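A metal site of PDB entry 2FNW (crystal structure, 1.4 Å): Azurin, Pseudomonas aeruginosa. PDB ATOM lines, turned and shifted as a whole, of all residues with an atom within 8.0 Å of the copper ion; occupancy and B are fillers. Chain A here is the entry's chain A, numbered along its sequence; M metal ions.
A ring nitrogen (NE2) of His 46 is in hydrogen-bond range of the backbone carbonyl oxygen (O) of Asn 10 (2.7 Å).
NE2 of His 117 sits close to SD of Met 44.
The side-chain sulfur (SG) of Cys 112 lies close to the backbone NH (N) of Asn 47, at 3.4 Å.
The backbone NH (N) of Cys 112 sits at hydrogen-bond distance from the backbone carbonyl oxygen (O) of Met 121 (3.3 Å).
A ring nitrogen (NE2) of His 46 sits close to the backbone carbonyl oxygen (O) of Met 44 (3.4 Å).
The side-chain sulfur (SD) of Met 121 lies close to a ring nitrogen (ND1) of His 117 (3.7 Å).
SG of Cys 112 sits close to N of Phe 114.
N of Ile 87 sits at hydrogen-bond distance from O of His 46, 2.9 Å away.
Gly 45 touches the copper ion (O to CU, 3.1 Å).
Phe 114 touches the copper ion (CB to CU, 3.9 Å).
Met 121 touches the copper ion (SD to CU, 3.2 Å).
ND1 of His 117 binds the copper ion.
ND1 of His 46 binds the copper ion (2.1 Å).
The copper ion is bound by SG of Cys 112 (2.2 Å).
The copper ion has three donor atoms within binding distance.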
ATOM      1  N   GLY A   9       1.016 -13.707 -17.279  1.00  0.00           N
ATOM      2  CA  GLY A   9       2.426 -13.867 -16.946  1.00  0.00           C
ATOM      3  C   GLY A   9       2.654 -12.948 -15.737  1.00  0.00           C
ATOM      4  O   GLY A   9       2.288 -11.803 -15.818  1.00  0.00           O
ATOM      5  N   ASN A  10       3.237 -13.452 -14.666  1.00  0.00           N
ATOM      6  CA  ASN A  10       3.262 -12.631 -13.432  1.00  0.00           C
ATOM      7  C   ASN A  10       4.677 -12.311 -13.024  1.00  0.00           C
ATOM      8  O   ASN A  10       5.660 -12.619 -13.703  1.00  0.00           O
ATOM      9  CB  ASN A  10       2.498 -13.407 -12.373  1.00  0.00           C
ATOM     10  CG  ASN A  10       3.197 -14.695 -12.002  1.00  0.00           C
ATOM     11  OD1 ASN A  10       4.373 -14.951 -12.310  1.00  0.00           O
ATOM     12  ND2 ASN A  10       2.520 -15.604 -11.282  1.00  0.00           N
ATOM     13  N   MET A  13       7.703 -14.854 -12.801  1.00  0.00           N
ATOM     14  CA  MET A  13       8.195 -15.454 -14.045  1.00  0.00           C
ATOM     15  C   MET A  13       7.484 -16.742 -14.390  1.00  0.00           C
ATOM     16  O   MET A  13       8.052 -17.724 -14.821  1.00  0.00           O
ATOM     17  CB  MET A  13       9.687 -15.714 -13.910  1.00  0.00           C
ATOM     18  CG  MET A  13      10.420 -15.730 -15.235  1.00  0.00           C
ATOM     19  SD  MET A  13      12.171 -16.074 -14.998  1.00  0.00           S
ATOM     20  CE  MET A  13      12.599 -14.818 -13.809  1.00  0.00           C
ATOM     21  N   GLN A  14       6.168 -16.712 -14.290  1.00  0.00           N
ATOM     22  CA  GLN A  14       5.335 -17.866 -14.624  1.00  0.00           C
ATOM     23  C   GLN A  14       4.186 -17.525 -15.568  1.00  0.00           C
ATOM     24  O   GLN A  14       3.560 -16.499 -15.361  1.00  0.00           O
ATOM     25  CB  GLN A  14       4.714 -18.447 -13.339  1.00  0.00           C
ATOM     26  CG  GLN A  14       5.719 -19.095 -12.407  1.00  0.00           C
ATOM     27  CD  GLN A  14       5.997 -20.569 -12.628  1.00  0.00           C
ATOM     28  OE1 GLN A  14       5.376 -21.219 -13.462  1.00  0.00           O
ATOM     29  NE2 GLN A  14       6.964 -21.133 -11.891  1.00  0.00           N
ATOM     30  N   PHE A  15       3.924 -18.386 -16.543  1.00  0.00           N
ATOM     31  CA  PHE A  15       2.597 -18.339 -17.184  1.00  0.00           C
ATOM     32  C   PHE A  15       1.598 -19.110 -16.342  1.00  0.00           C
ATOM     33  O   PHE A  15       2.002 -20.046 -15.657  1.00  0.00           O
ATOM     34  CB  PHE A  15       2.556 -18.959 -18.586  1.00  0.00           C
ATOM     35  CG  PHE A  15       3.244 -18.170 -19.682  1.00  0.00           C
ATOM     36  CD1 PHE A  15       2.895 -16.863 -19.926  1.00  0.00           C
ATOM     37  CD2 PHE A  15       4.203 -18.783 -20.479  1.00  0.00           C
ATOM     38  CE1 PHE A  15       3.489 -16.155 -20.973  1.00  0.00           C
ATOM     39  CE2 PHE A  15       4.825 -18.057 -21.477  1.00  0.00           C
ATOM     40  CZ  PHE A  15       4.475 -16.738 -21.712  1.00  0.00           C
ATOM     41  N   LEU A  33      -3.045 -12.018 -23.336  1.00  0.00           N
ATOM     42  CA  LEU A  33      -1.979 -12.050 -22.338  1.00  0.00           C
ATOM     43  C   LEU A  33      -2.095 -10.845 -21.407  1.00  0.00           C
ATOM     44  O   LEU A  33      -2.130  -9.686 -21.760  1.00  0.00           O
ATOM     45  CB  LEU A  33      -0.571 -12.044 -22.925  1.00  0.00           C
ATOM     46  CG  LEU A  33       0.615 -11.994 -21.950  1.00  0.00           C
ATOM     47  CD1 LEU A  33       0.748 -13.314 -21.204  1.00  0.00           C
ATOM     48  CD2 LEU A  33       1.895 -11.615 -22.674  1.00  0.00           C
ATOM     49  N   HIS A  35      -0.332  -9.106 -17.795  1.00  0.00           N
ATOM     50  CA  HIS A  35       0.819  -9.167 -16.877  1.00  0.00           C
ATOM     51  C   HIS A  35       0.510  -8.492 -15.548  1.00  0.00           C
ATOM     52  O   HIS A  35       0.883  -7.340 -15.353  1.00  0.00           O
ATOM     53  CB  HIS A  35       2.050  -8.492 -17.537  1.00  0.00           C
ATOM     54  CG  HIS A  35       3.308  -8.566 -16.729  1.00  0.00           C
ATOM     55  ND1 HIS A  35       3.491  -8.926 -15.424  1.00  0.00           N
ATOM     56  CD2 HIS A  35       4.540  -8.269 -17.226  1.00  0.00           C
ATOM     57  CE1 HIS A  35       4.779  -8.857 -15.111  1.00  0.00           C
ATOM     58  NE2 HIS A  35       5.422  -8.467 -16.182  1.00  0.00           N
ATOM     59  N   VAL A  43      12.414  -4.888 -16.221  1.00  0.00           N
ATOM     60  CA  VAL A  43      12.875  -5.852 -15.216  1.00  0.00           C
ATOM     61  C   VAL A  43      12.274  -7.225 -15.429  1.00  0.00           C
ATOM     62  O   VAL A  43      12.954  -8.247 -15.275  1.00  0.00           O
ATOM     63  CB  VAL A  43      12.530  -5.333 -13.806  1.00  0.00           C
ATOM     64  CG1 VAL A  43      12.872  -6.364 -12.740  1.00  0.00           C
ATOM     65  CG2 VAL A  43      13.209  -4.007 -13.525  1.00  0.00           C
ATOM     66  N   MET A  44      10.991  -7.290 -15.828  1.00  0.00           N
ATOM     67  CA  MET A  44      10.240  -8.548 -15.857  1.00  0.00           C
ATOM     68  C   MET A  44       9.185  -8.603 -16.951  1.00  0.00           C
ATOM     69  O   MET A  44       8.092  -9.205 -16.810  1.00  0.00           O
ATOM     70  CB  MET A  44       9.569  -8.760 -14.498  1.00  0.00           C
ATOM     71  CG  MET A  44       8.840 -10.064 -14.293  1.00  0.00           C
ATOM     72  SD  MET A  44       9.864 -11.517 -14.205  1.00  0.00           S
ATOM     73  CE  MET A  44      10.782 -11.250 -12.695  1.00  0.00           C
ATOM     74  N   GLY A  45       9.485  -7.966 -18.076  1.00  0.00           N
ATOM     75  CA  GLY A  45       8.549  -7.930 -19.229  1.00  0.00           C
ATOM     76  C   GLY A  45       8.262  -9.350 -19.717  1.00  0.00           C
ATOM     77  O   GLY A  45       9.125 -10.218 -19.662  1.00  0.00           O
ATOM     78  N   HIS A  46       7.040  -9.574 -20.159  1.00  0.00           N
ATOM     79  CA  HIS A  46       6.671 -10.879 -20.678  1.00  0.00           C
ATOM     80  C   HIS A  46       6.064 -10.770 -22.073  1.00  0.00           C
ATOM     81  O   HIS A  46       5.344  -9.808 -22.327  1.00  0.00           O
ATOM     82  CB  HIS A  46       5.603 -11.575 -19.834  1.00  0.00           C
ATOM     83  CG  HIS A  46       6.072 -11.873 -18.440  1.00  0.00           C
ATOM     84  ND1 HIS A  46       7.313 -12.392 -18.193  1.00  0.00           N
ATOM     85  CD2 HIS A  46       5.485 -11.709 -17.233  1.00  0.00           C
ATOM     86  CE1 HIS A  46       7.452 -12.534 -16.885  1.00  0.00           C
ATOM     87  NE2 HIS A  46       6.371 -12.148 -16.294  1.00  0.00           N
ATOM     88  N   ASN A  47       6.314 -11.717 -22.965  1.00  0.00           N
ATOM     89  CA  ASN A  47       5.528 -11.779 -24.206  1.00  0.00           C
ATOM     90  C   ASN A  47       5.044 -13.250 -24.302  1.00  0.00           C
ATOM     91  O   ASN A  47       5.360 -14.072 -23.462  1.00  0.00           O
ATOM     92  CB  ASN A  47       6.236 -11.381 -25.512  1.00  0.00           C
ATOM     93  CG  ASN A  47       7.587 -12.044 -25.740  1.00  0.00           C
ATOM     94  OD1 ASN A  47       7.902 -13.018 -25.051  1.00  0.00           O
ATOM     95  ND2 ASN A  47       8.463 -11.529 -26.612  1.00  0.00           N
ATOM     96  N   TRP A  48       4.228 -13.454 -25.329  1.00  0.00           N
ATOM     97  CA  TRP A  48       3.763 -14.800 -25.643  1.00  0.00           C
ATOM     98  C   TRP A  48       4.109 -15.030 -27.113  1.00  0.00           C
ATOM     99  O   TRP A  48       3.597 -14.261 -27.929  1.00  0.00           O
ATOM    100  CB  TRP A  48       2.257 -14.930 -25.403  1.00  0.00           C
ATOM    101  CG  TRP A  48       1.723 -16.330 -25.596  1.00  0.00           C
ATOM    102  CD1 TRP A  48       1.632 -17.324 -24.646  1.00  0.00           C
ATOM    103  CD2 TRP A  48       1.207 -16.885 -26.785  1.00  0.00           C
ATOM    104  NE1 TRP A  48       1.081 -18.448 -25.221  1.00  0.00           N
ATOM    105  CE2 TRP A  48       0.812 -18.221 -26.549  1.00  0.00           C
ATOM    106  CE3 TRP A  48       1.045 -16.352 -28.092  1.00  0.00           C
ATOM    107  CZ2 TRP A  48       0.257 -19.076 -27.518  1.00  0.00           C
ATOM    108  CZ3 TRP A  48       0.499 -17.205 -29.038  1.00  0.00           C
ATOM    109  CH2 TRP A  48       0.102 -18.519 -28.785  1.00  0.00           C
ATOM    110  N   LEU A  86       5.932  -7.300 -25.930  1.00  0.00           N
ATOM    111  CA  LEU A  86       6.402  -7.441 -24.564  1.00  0.00           C
ATOM    112  C   LEU A  86       5.640  -6.457 -23.705  1.00  0.00           C
ATOM    113  O   LEU A  86       5.528  -5.286 -24.095  1.00  0.00           O
ATOM    114  CB  LEU A  86       7.916  -7.155 -24.529  1.00  0.00           C
ATOM    115  CG  LEU A  86       8.729  -7.650 -23.342  1.00  0.00           C
ATOM    116  CD1 LEU A  86       8.996  -9.142 -23.401  1.00  0.00           C
ATOM    117  CD2 LEU A  86      10.099  -6.958 -23.268  1.00  0.00           C
ATOM    118  N   ILE A  87       5.122  -6.973 -22.584  1.00  0.00           N
ATOM    119  CA  ILE A  87       4.410  -6.074 -21.679  1.00  0.00           C
ATOM    120  C   ILE A  87       4.994  -6.104 -20.283  1.00  0.00           C
ATOM    121  O   ILE A  87       5.427  -7.118 -19.786  1.00  0.00           O
ATOM    122  CB  ILE A  87       2.930  -6.455 -21.622  1.00  0.00           C
ATOM    123  CG1 ILE A  87       2.714  -7.937 -21.261  1.00  0.00           C
ATOM    124  CG2 ILE A  87       2.303  -6.047 -22.957  1.00  0.00           C
ATOM    125  CD1 ILE A  87       1.267  -8.309 -20.968  1.00  0.00           C
ATOM    126  N   PHE A 111       6.137 -19.503 -25.476  1.00  0.00           N
ATOM    127  CA  PHE A 111       7.190 -19.191 -24.518  1.00  0.00           C
ATOM    128  C   PHE A 111       7.262 -17.653 -24.517  1.00  0.00           C
ATOM    129  O   PHE A 111       6.687 -16.996 -25.356  1.00  0.00           O
ATOM    130  CB  PHE A 111       8.554 -19.781 -24.885  1.00  0.00           C
ATOM    131  CG  PHE A 111       8.790 -19.696 -26.405  1.00  0.00           C
ATOM    132  CD1 PHE A 111       8.301 -20.672 -27.267  1.00  0.00           C
ATOM    133  CD2 PHE A 111       9.471 -18.603 -26.897  1.00  0.00           C
ATOM    134  CE1 PHE A 111       8.490 -20.525 -28.640  1.00  0.00           C
ATOM    135  CE2 PHE A 111       9.681 -18.450 -28.253  1.00  0.00           C
ATOM    136  CZ  PHE A 111       9.178 -19.434 -29.096  1.00  0.00           C
ATOM    137  N   CYS A 112       7.957 -17.124 -23.553  1.00  0.00           N
ATOM    138  CA  CYS A 112       8.372 -15.757 -23.387  1.00  0.00           C
ATOM    139  C   CYS A 112       9.836 -15.654 -23.759  1.00  0.00           C
ATOM    140  O   CYS A 112      10.570 -16.568 -23.381  1.00  0.00           O
ATOM    141  CB  CYS A 112       8.253 -15.357 -21.892  1.00  0.00           C
ATOM    142  SG  CYS A 112       8.765 -13.647 -21.672  1.00  0.00           S
ATOM    143  N   THR A 113      10.213 -14.604 -24.484  1.00  0.00           N
ATOM    144  CA  THR A 113      11.613 -14.555 -24.907  1.00  0.00           C
ATOM    145  C   THR A 113      12.394 -13.551 -24.097  1.00  0.00           C
ATOM    146  O   THR A 113      13.569 -13.276 -24.374  1.00  0.00           O
ATOM    147  CB  THR A 113      11.707 -14.207 -26.423  1.00  0.00           C
ATOM    148  OG1 THR A 113      11.076 -12.951 -26.653  1.00  0.00           O
ATOM    149  CG2 THR A 113      10.966 -15.232 -27.318  1.00  0.00           C
ATOM    150  N   PHE A 114      11.790 -12.921 -23.065  1.00  0.00           N
ATOM    151  CA  PHE A 114      12.659 -12.108 -22.240  1.00  0.00           C
ATOM    152  C   PHE A 114      13.782 -12.946 -21.665  1.00  0.00           C
ATOM    153  O   PHE A 114      13.581 -14.090 -21.240  1.00  0.00           O
ATOM    154  CB  PHE A 114      11.756 -11.490 -21.155  1.00  0.00           C
ATOM    155  CG  PHE A 114      12.362 -10.310 -20.450  1.00  0.00           C
ATOM    156  CD1 PHE A 114      13.259 -10.560 -19.397  1.00  0.00           C
ATOM    157  CD2 PHE A 114      12.047  -9.021 -20.829  1.00  0.00           C
ATOM    158  CE1 PHE A 114      13.812  -9.467 -18.747  1.00  0.00           C
ATOM    159  CE2 PHE A 114      12.585  -7.948 -20.155  1.00  0.00           C
ATOM    160  CZ  PHE A 114      13.480  -8.177 -19.128  1.00  0.00           C
ATOM    161  N   PRO A 115      15.001 -12.417 -21.663  1.00  0.00           N
ATOM    162  CA  PRO A 115      16.148 -13.253 -21.272  1.00  0.00           C
ATOM    163  C   PRO A 115      15.953 -14.017 -19.972  1.00  0.00           C
ATOM    164  O   PRO A 115      15.659 -13.498 -18.879  1.00  0.00           O
ATOM    165  CB  PRO A 115      17.250 -12.203 -21.053  1.00  0.00           C
ATOM    166  CG  PRO A 115      16.852 -11.009 -21.838  1.00  0.00           C
ATOM    167  CD  PRO A 115      15.347 -11.031 -21.957  1.00  0.00           C
ATOM    168  N   GLY A 116      16.125 -15.330 -20.076  1.00  0.00           N
ATOM    169  CA  GLY A 116      16.050 -16.247 -18.969  1.00  0.00           C
ATOM    170  C   GLY A 116      14.659 -16.736 -18.670  1.00  0.00           C
ATOM    171  O   GLY A 116      14.430 -17.675 -17.910  1.00  0.00           O
ATOM    172  N   HIS A 117      13.631 -16.104 -19.248  1.00  0.00           N
ATOM    173  CA  HIS A 117      12.308 -16.503 -18.734  1.00  0.00           C
ATOM    174  C   HIS A 117      11.829 -17.851 -19.266  1.00  0.00           C
ATOM    175  O   HIS A 117      10.987 -18.497 -18.637  1.00  0.00           O
ATOM    176  CB  HIS A 117      11.279 -15.441 -19.114  1.00  0.00           C
ATOM    177  CG  HIS A 117      11.397 -14.162 -18.358  1.00  0.00           C
ATOM    178  ND1 HIS A 117      10.339 -13.281 -18.300  1.00  0.00           N
ATOM    179  CD2 HIS A 117      12.380 -13.605 -17.642  1.00  0.00           C
ATOM    180  CE1 HIS A 117      10.649 -12.219 -17.578  1.00  0.00           C
ATOM    181  NE2 HIS A 117      11.902 -12.412 -17.162  1.00  0.00           N
ATOM    182  N   SER A 118      12.343 -18.237 -20.426  1.00  0.00           N
ATOM    183  CA  SER A 118      11.796 -19.418 -21.088  1.00  0.00           C
ATOM    184  C   SER A 118      12.158 -20.688 -20.348  1.00  0.00           C
ATOM    185  O   SER A 118      11.523 -21.712 -20.610  1.00  0.00           O
ATOM    186  CB  SER A 118      12.244 -19.485 -22.551  1.00  0.00           C
ATOM    187  OG  SER A 118      13.620 -19.744 -22.603  1.00  0.00           O
ATOM    188  N   MET A 121       8.864 -20.152 -18.497  1.00  0.00           N
ATOM    189  CA  MET A 121       7.664 -19.667 -19.204  1.00  0.00           C
ATOM    190  C   MET A 121       7.644 -20.281 -20.588  1.00  0.00           C
ATOM    191  O   MET A 121       8.149 -19.727 -21.561  1.00  0.00           O
ATOM    192  CB  MET A 121       7.693 -18.118 -19.278  1.00  0.00           C
ATOM    193  CG  MET A 121       7.630 -17.499 -17.875  1.00  0.00           C
ATOM    194  SD  MET A 121       7.574 -15.702 -17.839  1.00  0.00           S
ATOM    195  CE  MET A 121       5.922 -15.489 -18.462  1.00  0.00           C
HETATM  196 CU    CU M   1       8.668 -13.239 -19.526  1.00  0.00          CU
